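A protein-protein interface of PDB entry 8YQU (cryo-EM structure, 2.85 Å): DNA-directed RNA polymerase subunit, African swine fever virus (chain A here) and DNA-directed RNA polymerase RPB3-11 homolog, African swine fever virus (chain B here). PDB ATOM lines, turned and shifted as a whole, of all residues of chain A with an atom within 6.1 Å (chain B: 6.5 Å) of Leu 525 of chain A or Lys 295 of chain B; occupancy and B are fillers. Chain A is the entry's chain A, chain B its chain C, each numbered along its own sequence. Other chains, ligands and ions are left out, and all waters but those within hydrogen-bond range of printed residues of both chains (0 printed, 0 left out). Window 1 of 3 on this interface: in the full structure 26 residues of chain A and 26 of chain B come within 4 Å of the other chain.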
ATOM      1  N   ASN A 523      13.736 -10.352 -22.160  1.00  0.00           N
ATOM      2  CA  ASN A 523      12.798 -11.000 -21.258  1.00  0.00           C
ATOM      3  C   ASN A 523      12.987 -12.515 -21.301  1.00  0.00           C
ATOM      4  O   ASN A 523      13.833 -13.046 -22.027  1.00  0.00           O
ATOM      5  CB  ASN A 523      11.362 -10.606 -21.602  1.00  0.00           C
ATOM      6  CG  ASN A 523      11.032 -10.808 -23.065  1.00  0.00           C
ATOM      7  OD1 ASN A 523      11.843 -11.322 -23.832  1.00  0.00           O
ATOM      8  ND2 ASN A 523       9.832 -10.404 -23.460  1.00  0.00           N
ATOM      9  N   LYS A 524      12.190 -13.223 -20.498  1.00  0.00           N
ATOM     10  CA  LYS A 524      12.290 -14.678 -20.448  1.00  0.00           C
ATOM     11  C   LYS A 524      11.926 -15.307 -21.787  1.00  0.00           C
ATOM     12  O   LYS A 524      12.557 -16.281 -22.211  1.00  0.00           O
ATOM     13  CB  LYS A 524      11.394 -15.223 -19.338  1.00  0.00           C
ATOM     14  CG  LYS A 524      11.282 -16.736 -19.317  1.00  0.00           C
ATOM     15  CD  LYS A 524      10.367 -17.201 -18.200  1.00  0.00           C
ATOM     16  CE  LYS A 524      10.126 -18.696 -18.274  1.00  0.00           C
ATOM     17  NZ  LYS A 524       9.307 -19.173 -17.129  1.00  0.00           N
ATOM     18  N   LEU A 525      10.909 -14.766 -22.463  1.00  0.00           N
ATOM     19  CA  LEU A 525      10.459 -15.353 -23.720  1.00  0.00           C
ATOM     20  C   LEU A 525      11.548 -15.301 -24.784  1.00  0.00           C
ATOM     21  O   LEU A 525      11.766 -16.279 -25.508  1.00  0.00           O
ATOM     22  CB  LEU A 525       9.201 -14.638 -24.210  1.00  0.00           C
ATOM     23  CG  LEU A 525       8.574 -15.205 -25.482  1.00  0.00           C
ATOM     24  CD1 LEU A 525       8.157 -16.646 -25.260  1.00  0.00           C
ATOM     25  CD2 LEU A 525       7.392 -14.360 -25.923  1.00  0.00           C
ATOM     26  N   HIS A 526      12.242 -14.167 -24.898  1.00  0.00           N
ATOM     27  CA  HIS A 526      13.301 -14.044 -25.890  1.00  0.00           C
ATOM     28  C   HIS A 526      14.604 -14.688 -25.440  1.00  0.00           C
ATOM     29  O   HIS A 526      15.470 -14.950 -26.280  1.00  0.00           O
ATOM     30  CB  HIS A 526      13.536 -12.572 -26.229  1.00  0.00           C
ATOM     31  CG  HIS A 526      12.402 -11.940 -26.972  1.00  0.00           C
ATOM     32  ND1 HIS A 526      11.322 -11.367 -26.336  1.00  0.00           N
ATOM     33  CD2 HIS A 526      12.177 -11.795 -28.300  1.00  0.00           C
ATOM     34  CE1 HIS A 526      10.482 -10.896 -27.240  1.00  0.00           C
ATOM     35  NE2 HIS A 526      10.978 -11.142 -28.439  1.00  0.00           N
ATOM     36  N   ALA A 527      14.765 -14.943 -24.140  1.00  0.00           N
ATOM     37  CA  ALA A 527      15.928 -15.691 -23.679  1.00  0.00           C
ATOM     38  C   ALA A 527      15.807 -17.165 -24.043  1.00  0.00           C
ATOM     39  O   ALA A 527      16.801 -17.805 -24.407  1.00  0.00           O
ATOM     40  CB  ALA A 527      16.101 -15.520 -22.171  1.00  0.00           C
ATOM     41  N   MET A 528      14.597 -17.719 -23.947  1.00  0.00           N
ATOM     42  CA  MET A 528      14.374 -19.099 -24.362  1.00  0.00           C
ATOM     43  C   MET A 528      14.485 -19.255 -25.872  1.00  0.00           C
ATOM     44  O   MET A 528      14.916 -20.307 -26.356  1.00  0.00           O
ATOM     45  CB  MET A 528      13.006 -19.579 -23.884  1.00  0.00           C
ATOM     46  CG  MET A 528      12.871 -19.682 -22.378  1.00  0.00           C
ATOM     47  SD  MET A 528      11.385 -20.572 -21.886  1.00  0.00           S
ATOM     48  CE  MET A 528      10.118 -19.464 -22.494  1.00  0.00           C
ATOM     49  N   GLY A 529      14.100 -18.225 -26.630  1.00  0.00           N
ATOM     50  CA  GLY A 529      14.156 -18.300 -28.078  1.00  0.00           C
ATOM     51  C   GLY A 529      15.558 -18.378 -28.639  1.00  0.00           C
ATOM     52  O   GLY A 529      15.729 -18.757 -29.802  1.00  0.00           O
ATOM     53  N   LEU A 530      16.567 -18.019 -27.845  1.00  0.00           N
ATOM     54  CA  LEU A 530      17.948 -18.132 -28.291  1.00  0.00           C
ATOM     55  C   LEU A 530      18.468 -19.560 -28.224  1.00  0.00           C
ATOM     56  O   LEU A 530      19.479 -19.867 -28.864  1.00  0.00           O
ATOM     57  CB  LEU A 530      18.844 -17.216 -27.454  1.00  0.00           C
ATOM     58  CG  LEU A 530      19.245 -15.885 -28.092  1.00  0.00           C
ATOM     59  CD1 LEU A 530      18.019 -15.087 -28.499  1.00  0.00           C
ATOM     60  CD2 LEU A 530      20.108 -15.081 -27.137  1.00  0.00           C
ATOM     61  N   GLN A 532      16.461 -22.362 -28.872  1.00  0.00           N
ATOM     62  CA  GLN A 532      15.535 -23.252 -29.557  1.00  0.00           C
ATOM     63  C   GLN A 532      16.092 -23.786 -30.870  1.00  0.00           C
ATOM     64  O   GLN A 532      15.386 -24.511 -31.579  1.00  0.00           O
ATOM     65  CB  GLN A 532      14.203 -22.539 -29.804  1.00  0.00           C
ATOM     66  CG  GLN A 532      14.270 -21.417 -30.819  1.00  0.00           C
ATOM     67  CD  GLN A 532      12.976 -20.636 -30.898  1.00  0.00           C
ATOM     68  OE1 GLN A 532      12.066 -20.838 -30.095  1.00  0.00           O
ATOM     69  NE2 GLN A 532      12.883 -19.741 -31.873  1.00  0.00           N
ATOM     70  N   PRO A 546       7.866 -13.980 -16.400  1.00  0.00           N
ATOM     71  CA  PRO A 546       7.835 -13.475 -17.782  1.00  0.00           C
ATOM     72  C   PRO A 546       8.389 -12.070 -17.934  1.00  0.00           C
ATOM     73  O   PRO A 546       8.874 -11.728 -19.019  1.00  0.00           O
ATOM     74  CB  PRO A 546       6.346 -13.533 -18.141  1.00  0.00           C
ATOM     75  CG  PRO A 546       5.823 -14.646 -17.313  1.00  0.00           C
ATOM     76  CD  PRO A 546       6.581 -14.589 -16.014  1.00  0.00           C
ATOM     77  N   ARG B  52       0.667 -10.410 -30.907  1.00  0.00           N
ATOM     78  CA  ARG B  52       1.190 -10.220 -32.254  1.00  0.00           C
ATOM     79  C   ARG B  52       1.453 -11.537 -32.970  1.00  0.00           C
ATOM     80  O   ARG B  52       1.510 -11.554 -34.203  1.00  0.00           O
ATOM     81  CB  ARG B  52       2.460  -9.371 -32.199  1.00  0.00           C
ATOM     82  CG  ARG B  52       3.604  -9.996 -31.427  1.00  0.00           C
ATOM     83  CD  ARG B  52       4.766  -9.025 -31.333  1.00  0.00           C
ATOM     84  NE  ARG B  52       5.875  -9.562 -30.554  1.00  0.00           N
ATOM     85  CZ  ARG B  52       7.003  -8.907 -30.315  1.00  0.00           C
ATOM     86  NH1 ARG B  52       7.220  -7.700 -30.808  1.00  0.00           N
ATOM     87  NH2 ARG B  52       7.934  -9.477 -29.555  1.00  0.00           N
ATOM     88  N   ASP B 213       6.131  -6.329 -25.596  1.00  0.00           N
ATOM     89  CA  ASP B 213       5.067  -7.307 -25.829  1.00  0.00           C
ATOM     90  C   ASP B 213       3.815  -6.563 -26.267  1.00  0.00           C
ATOM     91  O   ASP B 213       2.864  -6.400 -25.493  1.00  0.00           O
ATOM     92  CB  ASP B 213       4.802  -8.145 -24.575  1.00  0.00           C
ATOM     93  CG  ASP B 213       3.908  -9.341 -24.849  1.00  0.00           C
ATOM     94  OD1 ASP B 213       3.555  -9.572 -26.026  1.00  0.00           O
ATOM     95  OD2 ASP B 213       3.556 -10.054 -23.886  1.00  0.00           O
ATOM     96  N   ILE B 290       1.852 -21.855 -37.075  1.00  0.00           N
ATOM     97  CA  ILE B 290       1.326 -22.736 -36.038  1.00  0.00           C
ATOM     98  C   ILE B 290       2.312 -22.860 -34.887  1.00  0.00           C
ATOM     99  O   ILE B 290       1.921 -22.845 -33.713  1.00  0.00           O
ATOM    100  CB  ILE B 290       0.975 -24.110 -36.638  1.00  0.00           C
ATOM    101  CG1 ILE B 290      -0.123 -23.961 -37.691  1.00  0.00           C
ATOM    102  CG2 ILE B 290       0.537 -25.073 -35.549  1.00  0.00           C
ATOM    103  CD1 ILE B 290      -1.386 -23.321 -37.163  1.00  0.00           C
ATOM    104  N   GLY B 291       3.604 -22.987 -35.197  1.00  0.00           N
ATOM    105  CA  GLY B 291       4.596 -23.113 -34.142  1.00  0.00           C
ATOM    106  C   GLY B 291       4.658 -21.887 -33.253  1.00  0.00           C
ATOM    107  O   GLY B 291       4.718 -21.996 -32.025  1.00  0.00           O
ATOM    108  N   ASN B 292       4.645 -20.698 -33.862  1.00  0.00           N
ATOM    109  CA  ASN B 292       4.679 -19.466 -33.085  1.00  0.00           C
ATOM    110  C   ASN B 292       3.418 -19.304 -32.249  1.00  0.00           C
ATOM    111  O   ASN B 292       3.491 -18.895 -31.084  1.00  0.00           O
ATOM    112  CB  ASN B 292       4.869 -18.267 -34.012  1.00  0.00           C
ATOM    113  CG  ASN B 292       5.618 -17.131 -33.346  1.00  0.00           C
ATOM    114  OD1 ASN B 292       6.629 -17.348 -32.680  1.00  0.00           O
ATOM    115  ND2 ASN B 292       5.124 -15.912 -33.524  1.00  0.00           N
ATOM    116  N   LEU B 293       2.252 -19.625 -32.819  1.00  0.00           N
ATOM    117  CA  LEU B 293       1.014 -19.553 -32.047  1.00  0.00           C
ATOM    118  C   LEU B 293       1.061 -20.496 -30.854  1.00  0.00           C
ATOM    119  O   LEU B 293       0.691 -20.123 -29.732  1.00  0.00           O
ATOM    120  CB  LEU B 293      -0.182 -19.881 -32.941  1.00  0.00           C
ATOM    121  CG  LEU B 293      -0.884 -18.711 -33.625  1.00  0.00           C
ATOM    122  CD1 LEU B 293      -1.899 -19.221 -34.630  1.00  0.00           C
ATOM    123  CD2 LEU B 293      -1.554 -17.826 -32.590  1.00  0.00           C
ATOM    124  N   LEU B 294       1.525 -21.728 -31.078  1.00  0.00           N
ATOM    125  CA  LEU B 294       1.603 -22.703 -30.000  1.00  0.00           C
ATOM    126  C   LEU B 294       2.553 -22.233 -28.909  1.00  0.00           C
ATOM    127  O   LEU B 294       2.222 -22.290 -27.719  1.00  0.00           O
ATOM    128  CB  LEU B 294       2.041 -24.061 -30.549  1.00  0.00           C
ATOM    129  CG  LEU B 294       0.968 -24.885 -31.262  1.00  0.00           C
ATOM    130  CD1 LEU B 294       1.556 -26.176 -31.804  1.00  0.00           C
ATOM    131  CD2 LEU B 294      -0.190 -25.172 -30.324  1.00  0.00           C
ATOM    132  N   LYS B 295       3.738 -21.752 -29.292  1.00  0.00           N
ATOM    133  CA  LYS B 295       4.693 -21.289 -28.291  1.00  0.00           C
ATOM    134  C   LYS B 295       4.122 -20.126 -27.494  1.00  0.00           C
ATOM    135  O   LYS B 295       4.208 -20.106 -26.261  1.00  0.00           O
ATOM    136  CB  LYS B 295       6.012 -20.879 -28.946  1.00  0.00           C
ATOM    137  CG  LYS B 295       7.056 -20.448 -27.924  1.00  0.00           C
ATOM    138  CD  LYS B 295       8.446 -20.340 -28.516  1.00  0.00           C
ATOM    139  CE  LYS B 295       8.665 -18.985 -29.165  1.00  0.00           C
ATOM    140  NZ  LYS B 295       8.851 -17.903 -28.168  1.00  0.00           N
ATOM    141  N   THR B 296       3.516 -19.156 -28.183  1.00  0.00           N
ATOM    142  CA  THR B 296       2.994 -17.979 -27.497  1.00  0.00           C
ATOM    143  C   THR B 296       1.892 -18.354 -26.516  1.00  0.00           C
ATOM    144  O   THR B 296       1.888 -17.889 -25.369  1.00  0.00           O
ATOM    145  CB  THR B 296       2.480 -16.966 -28.519  1.00  0.00           C
ATOM    146  OG1 THR B 296       3.553 -16.580 -29.387  1.00  0.00           O
ATOM    147  CG2 THR B 296       1.934 -15.734 -27.819  1.00  0.00           C
ATOM    148  N   TYR B 297       0.964 -19.216 -26.931  1.00  0.00           N
ATOM    149  CA  TYR B 297      -0.156 -19.534 -26.053  1.00  0.00           C
ATOM    150  C   TYR B 297       0.236 -20.484 -24.927  1.00  0.00           C
ATOM    151  O   TYR B 297      -0.310 -20.376 -23.823  1.00  0.00           O
ATOM    152  CB  TYR B 297      -1.315 -20.094 -26.872  1.00  0.00           C
ATOM    153  CG  TYR B 297      -2.171 -19.002 -27.467  1.00  0.00           C
ATOM    154  CD1 TYR B 297      -1.819 -18.392 -28.663  1.00  0.00           C
ATOM    155  CD2 TYR B 297      -3.322 -18.568 -26.826  1.00  0.00           C
ATOM    156  CE1 TYR B 297      -2.594 -17.389 -29.208  1.00  0.00           C
ATOM    157  CE2 TYR B 297      -4.104 -17.566 -27.363  1.00  0.00           C
ATOM    158  CZ  TYR B 297      -3.736 -16.980 -28.555  1.00  0.00           C
ATOM    159  OH  TYR B 297      -4.510 -15.980 -29.095  1.00  0.00           O
ATOM    160  N   ILE B 298       1.177 -21.402 -25.164  1.00  0.00           N
ATOM    161  CA  ILE B 298       1.688 -22.225 -24.072  1.00  0.00           C
ATOM    162  C   ILE B 298       2.433 -21.360 -23.064  1.00  0.00           C
ATOM    163  O   ILE B 298       2.297 -21.541 -21.848  1.00  0.00           O
ATOM    164  CB  ILE B 298       2.579 -23.355 -24.622  1.00  0.00           C
ATOM    165  CG1 ILE B 298       1.751 -24.337 -25.449  1.00  0.00           C
ATOM    166  CG2 ILE B 298       3.270 -24.092 -23.489  1.00  0.00           C
ATOM    167  CD1 ILE B 298       2.582 -25.195 -26.374  1.00  0.00           C
ATOM    168  N   TYR B 299       3.226 -20.403 -23.551  1.00  0.00           N
ATOM    169  CA  TYR B 299       3.951 -19.508 -22.659  1.00  0.00           C
ATOM    170  C   TYR B 299       2.995 -18.647 -21.844  1.00  0.00           C
ATOM    171  O   TYR B 299       3.226 -18.406 -20.653  1.00  0.00           O
ATOM    172  CB  TYR B 299       4.904 -18.637 -23.477  1.00  0.00           C
ATOM    173  CG  TYR B 299       5.761 -17.703 -22.662  1.00  0.00           C
ATOM    174  CD1 TYR B 299       6.734 -18.196 -21.805  1.00  0.00           C
ATOM    175  CD2 TYR B 299       5.609 -16.329 -22.762  1.00  0.00           C
ATOM    176  CE1 TYR B 299       7.525 -17.345 -21.064  1.00  0.00           C
ATOM    177  CE2 TYR B 299       6.396 -15.469 -22.025  1.00  0.00           C
ATOM    178  CZ  TYR B 299       7.351 -15.984 -21.178  1.00  0.00           C
ATOM    179  OH  TYR B 299       8.137 -15.130 -20.444  1.00  0.00           O
ATOM    180  N   GLU B 300       1.917 -18.169 -22.469  1.00  0.00           N
ATOM    181  CA  GLU B 300       0.906 -17.420 -21.729  1.00  0.00           C
ATOM    182  C   GLU B 300       0.221 -18.298 -20.689  1.00  0.00           C
ATOM    183  O   GLU B 300      -0.042 -17.850 -19.567  1.00  0.00           O
ATOM    184  CB  GLU B 300      -0.125 -16.833 -22.691  1.00  0.00           C
ATOM    185  CG  GLU B 300       0.394 -15.689 -23.541  1.00  0.00           C
ATOM    186  CD  GLU B 300      -0.676 -15.113 -24.447  1.00  0.00           C
ATOM    187  OE1 GLU B 300      -1.826 -15.595 -24.390  1.00  0.00           O
ATOM    188  OE2 GLU B 300      -0.366 -14.181 -25.218  1.00  0.00           O
ATOM    189  N   VAL B 308      10.219 -23.776 -23.907  1.00  0.00           N
ATOM    190  CA  VAL B 308       9.308 -23.963 -25.035  1.00  0.00           C
ATOM    191  C   VAL B 308       9.965 -23.392 -26.289  1.00  0.00           C
ATOM    192  O   VAL B 308      10.553 -22.307 -26.258  1.00  0.00           O
ATOM    193  CB  VAL B 308       7.927 -23.327 -24.767  1.00  0.00           C
ATOM    194  CG1 VAL B 308       8.030 -21.816 -24.619  1.00  0.00           C
ATOM    195  CG2 VAL B 308       6.947 -23.697 -25.867  1.00  0.00           C
ATOM    196  N   GLY B 309       9.893 -24.144 -27.379  1.00  0.00           N
ATOM    197  CA  GLY B 309      10.459 -23.704 -28.645  1.00  0.00           C
ATOM    198  C   GLY B 309       9.776 -24.394 -29.807  1.00  0.00           C
ATOM    199  O   GLY B 309       9.321 -25.531 -29.692  1.00  0.00           O
ATOM    200  N   TYR B 310       9.722 -23.697 -30.949  1.00  0.00           N
ATOM    201  CA  TYR B 310       8.920 -24.152 -32.085  1.00  0.00           C
ATOM    202  C   TYR B 310       9.753 -24.398 -33.340  1.00  0.00           C
ATOM    203  O   TYR B 310       9.267 -24.165 -34.449  1.00  0.00           O
ATOM    204  CB  TYR B 310       7.805 -23.145 -32.393  1.00  0.00           C
ATOM    205  CG  TYR B 310       8.269 -21.794 -32.910  1.00  0.00           C
ATOM    206  CD1 TYR B 310       8.584 -20.765 -32.040  1.00  0.00           C
ATOM    207  CD2 TYR B 310       8.326 -21.529 -34.274  1.00  0.00           C
ATOM    208  CE1 TYR B 310       8.993 -19.532 -32.514  1.00  0.00           C
ATOM    209  CE2 TYR B 310       8.731 -20.308 -34.754  1.00  0.00           C
ATOM    210  CZ  TYR B 310       9.061 -19.310 -33.870  1.00  0.00           C
ATOM    211  OH  TYR B 310       9.462 -18.086 -34.347  1.00  0.00           O
ATOM    212  N   LEU B 321       8.176 -28.790 -31.865  1.00  0.00           N
ATOM    213  CA  LEU B 321       7.842 -28.017 -30.677  1.00  0.00           C
ATOM    214  C   LEU B 321       8.299 -28.793 -29.449  1.00  0.00           C
ATOM    215  O   LEU B 321       7.799 -29.891 -29.182  1.00  0.00           O
ATOM    216  CB  LEU B 321       6.341 -27.739 -30.617  1.00  0.00           C
ATOM    217  CG  LEU B 321       5.787 -26.950 -29.428  1.00  0.00           C
ATOM    218  CD1 LEU B 321       6.191 -25.491 -29.497  1.00  0.00           C
ATOM    219  CD2 LEU B 321       4.276 -27.077 -29.373  1.00  0.00           C
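OD1 of Asn 523 of chain A sits at hydrogen-bond distance from ND1 of His 526 of chain A (2.6 Å). The side-chain hydroxyl (OH) of Tyr 310 of chain B lies close to the side-chain amide oxygen (OD1) of Asn 292 of chain B (3.4 Å).
Printed residues of chain A within 4 Å of Lys 295 of chain B: Leu 525 and Gln 532. Of the printed residues of chain A, Tyr 310 of chain B touches Gln 532 (3.8 Å). Of the printed residues of chain A, Val 308 of chain B touches Met 528. Of the printed residues of chain B, His 526 of chain A touches Arg 52 (3.6 Å). Printed residues of chain A within 4 Å of Arg 52 of chain B: His 526. Ala 527 of chain A touches none of the printed residues of chain B. The nearest residue of chain B that does not touch Leu 525 of chain A is Val 308 of chain B (5.2 Å).
The side-chain hydroxyl (OH) of Tyr 299 of chain B lies within hydrogen-bond range of the backbone NH (N) of Leu 525 of chain A, 3.4 Å away.
Printed residues of chain A that touch a printed residue of chain B: Lys 524, Leu 525, His 526, Met 528, Gln 532 and Pro 546. Hydrophobic or aromatic side chains of chain A within 4 Å of the printed part of chain B: Leu 525, His 526, Met 528 and Pro 546. Hydrophobic or aromatic side chains of chain B that line the printed part of chain A: Tyr 299, Val 308 and Tyr 310. Among the printed residues, no Asp or Glu carboxylate lies within 4 Å of a Lys or Arg side-chain nitrogen of the other chain.
OH of Tyr 299 of chain B touches CB of Lys 524 of chain A, 3.4 Å away. Lys 295 of chain B touches Leu 525 of chain A. His 526 of chain A touches Arg 52 of chain B (NE2 to NH2, 3.6 Å). Tyr 299 of chain B touches Met 528 of chain A. CG1 of Val 308 of chain B touches CE of Met 528 of chain A (3.8 Å). Lys 295 of chain B touches Gln 532 of chain A. Gln 532 of chain A touches Gly 309 of chain B. OE1 of Gln 532 of chain A touches N of Tyr 310 of chain B, 3.8 Å away. Pro 546 of chain A touches Tyr 299 of chain B (CA to OH, 3.1 Å).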
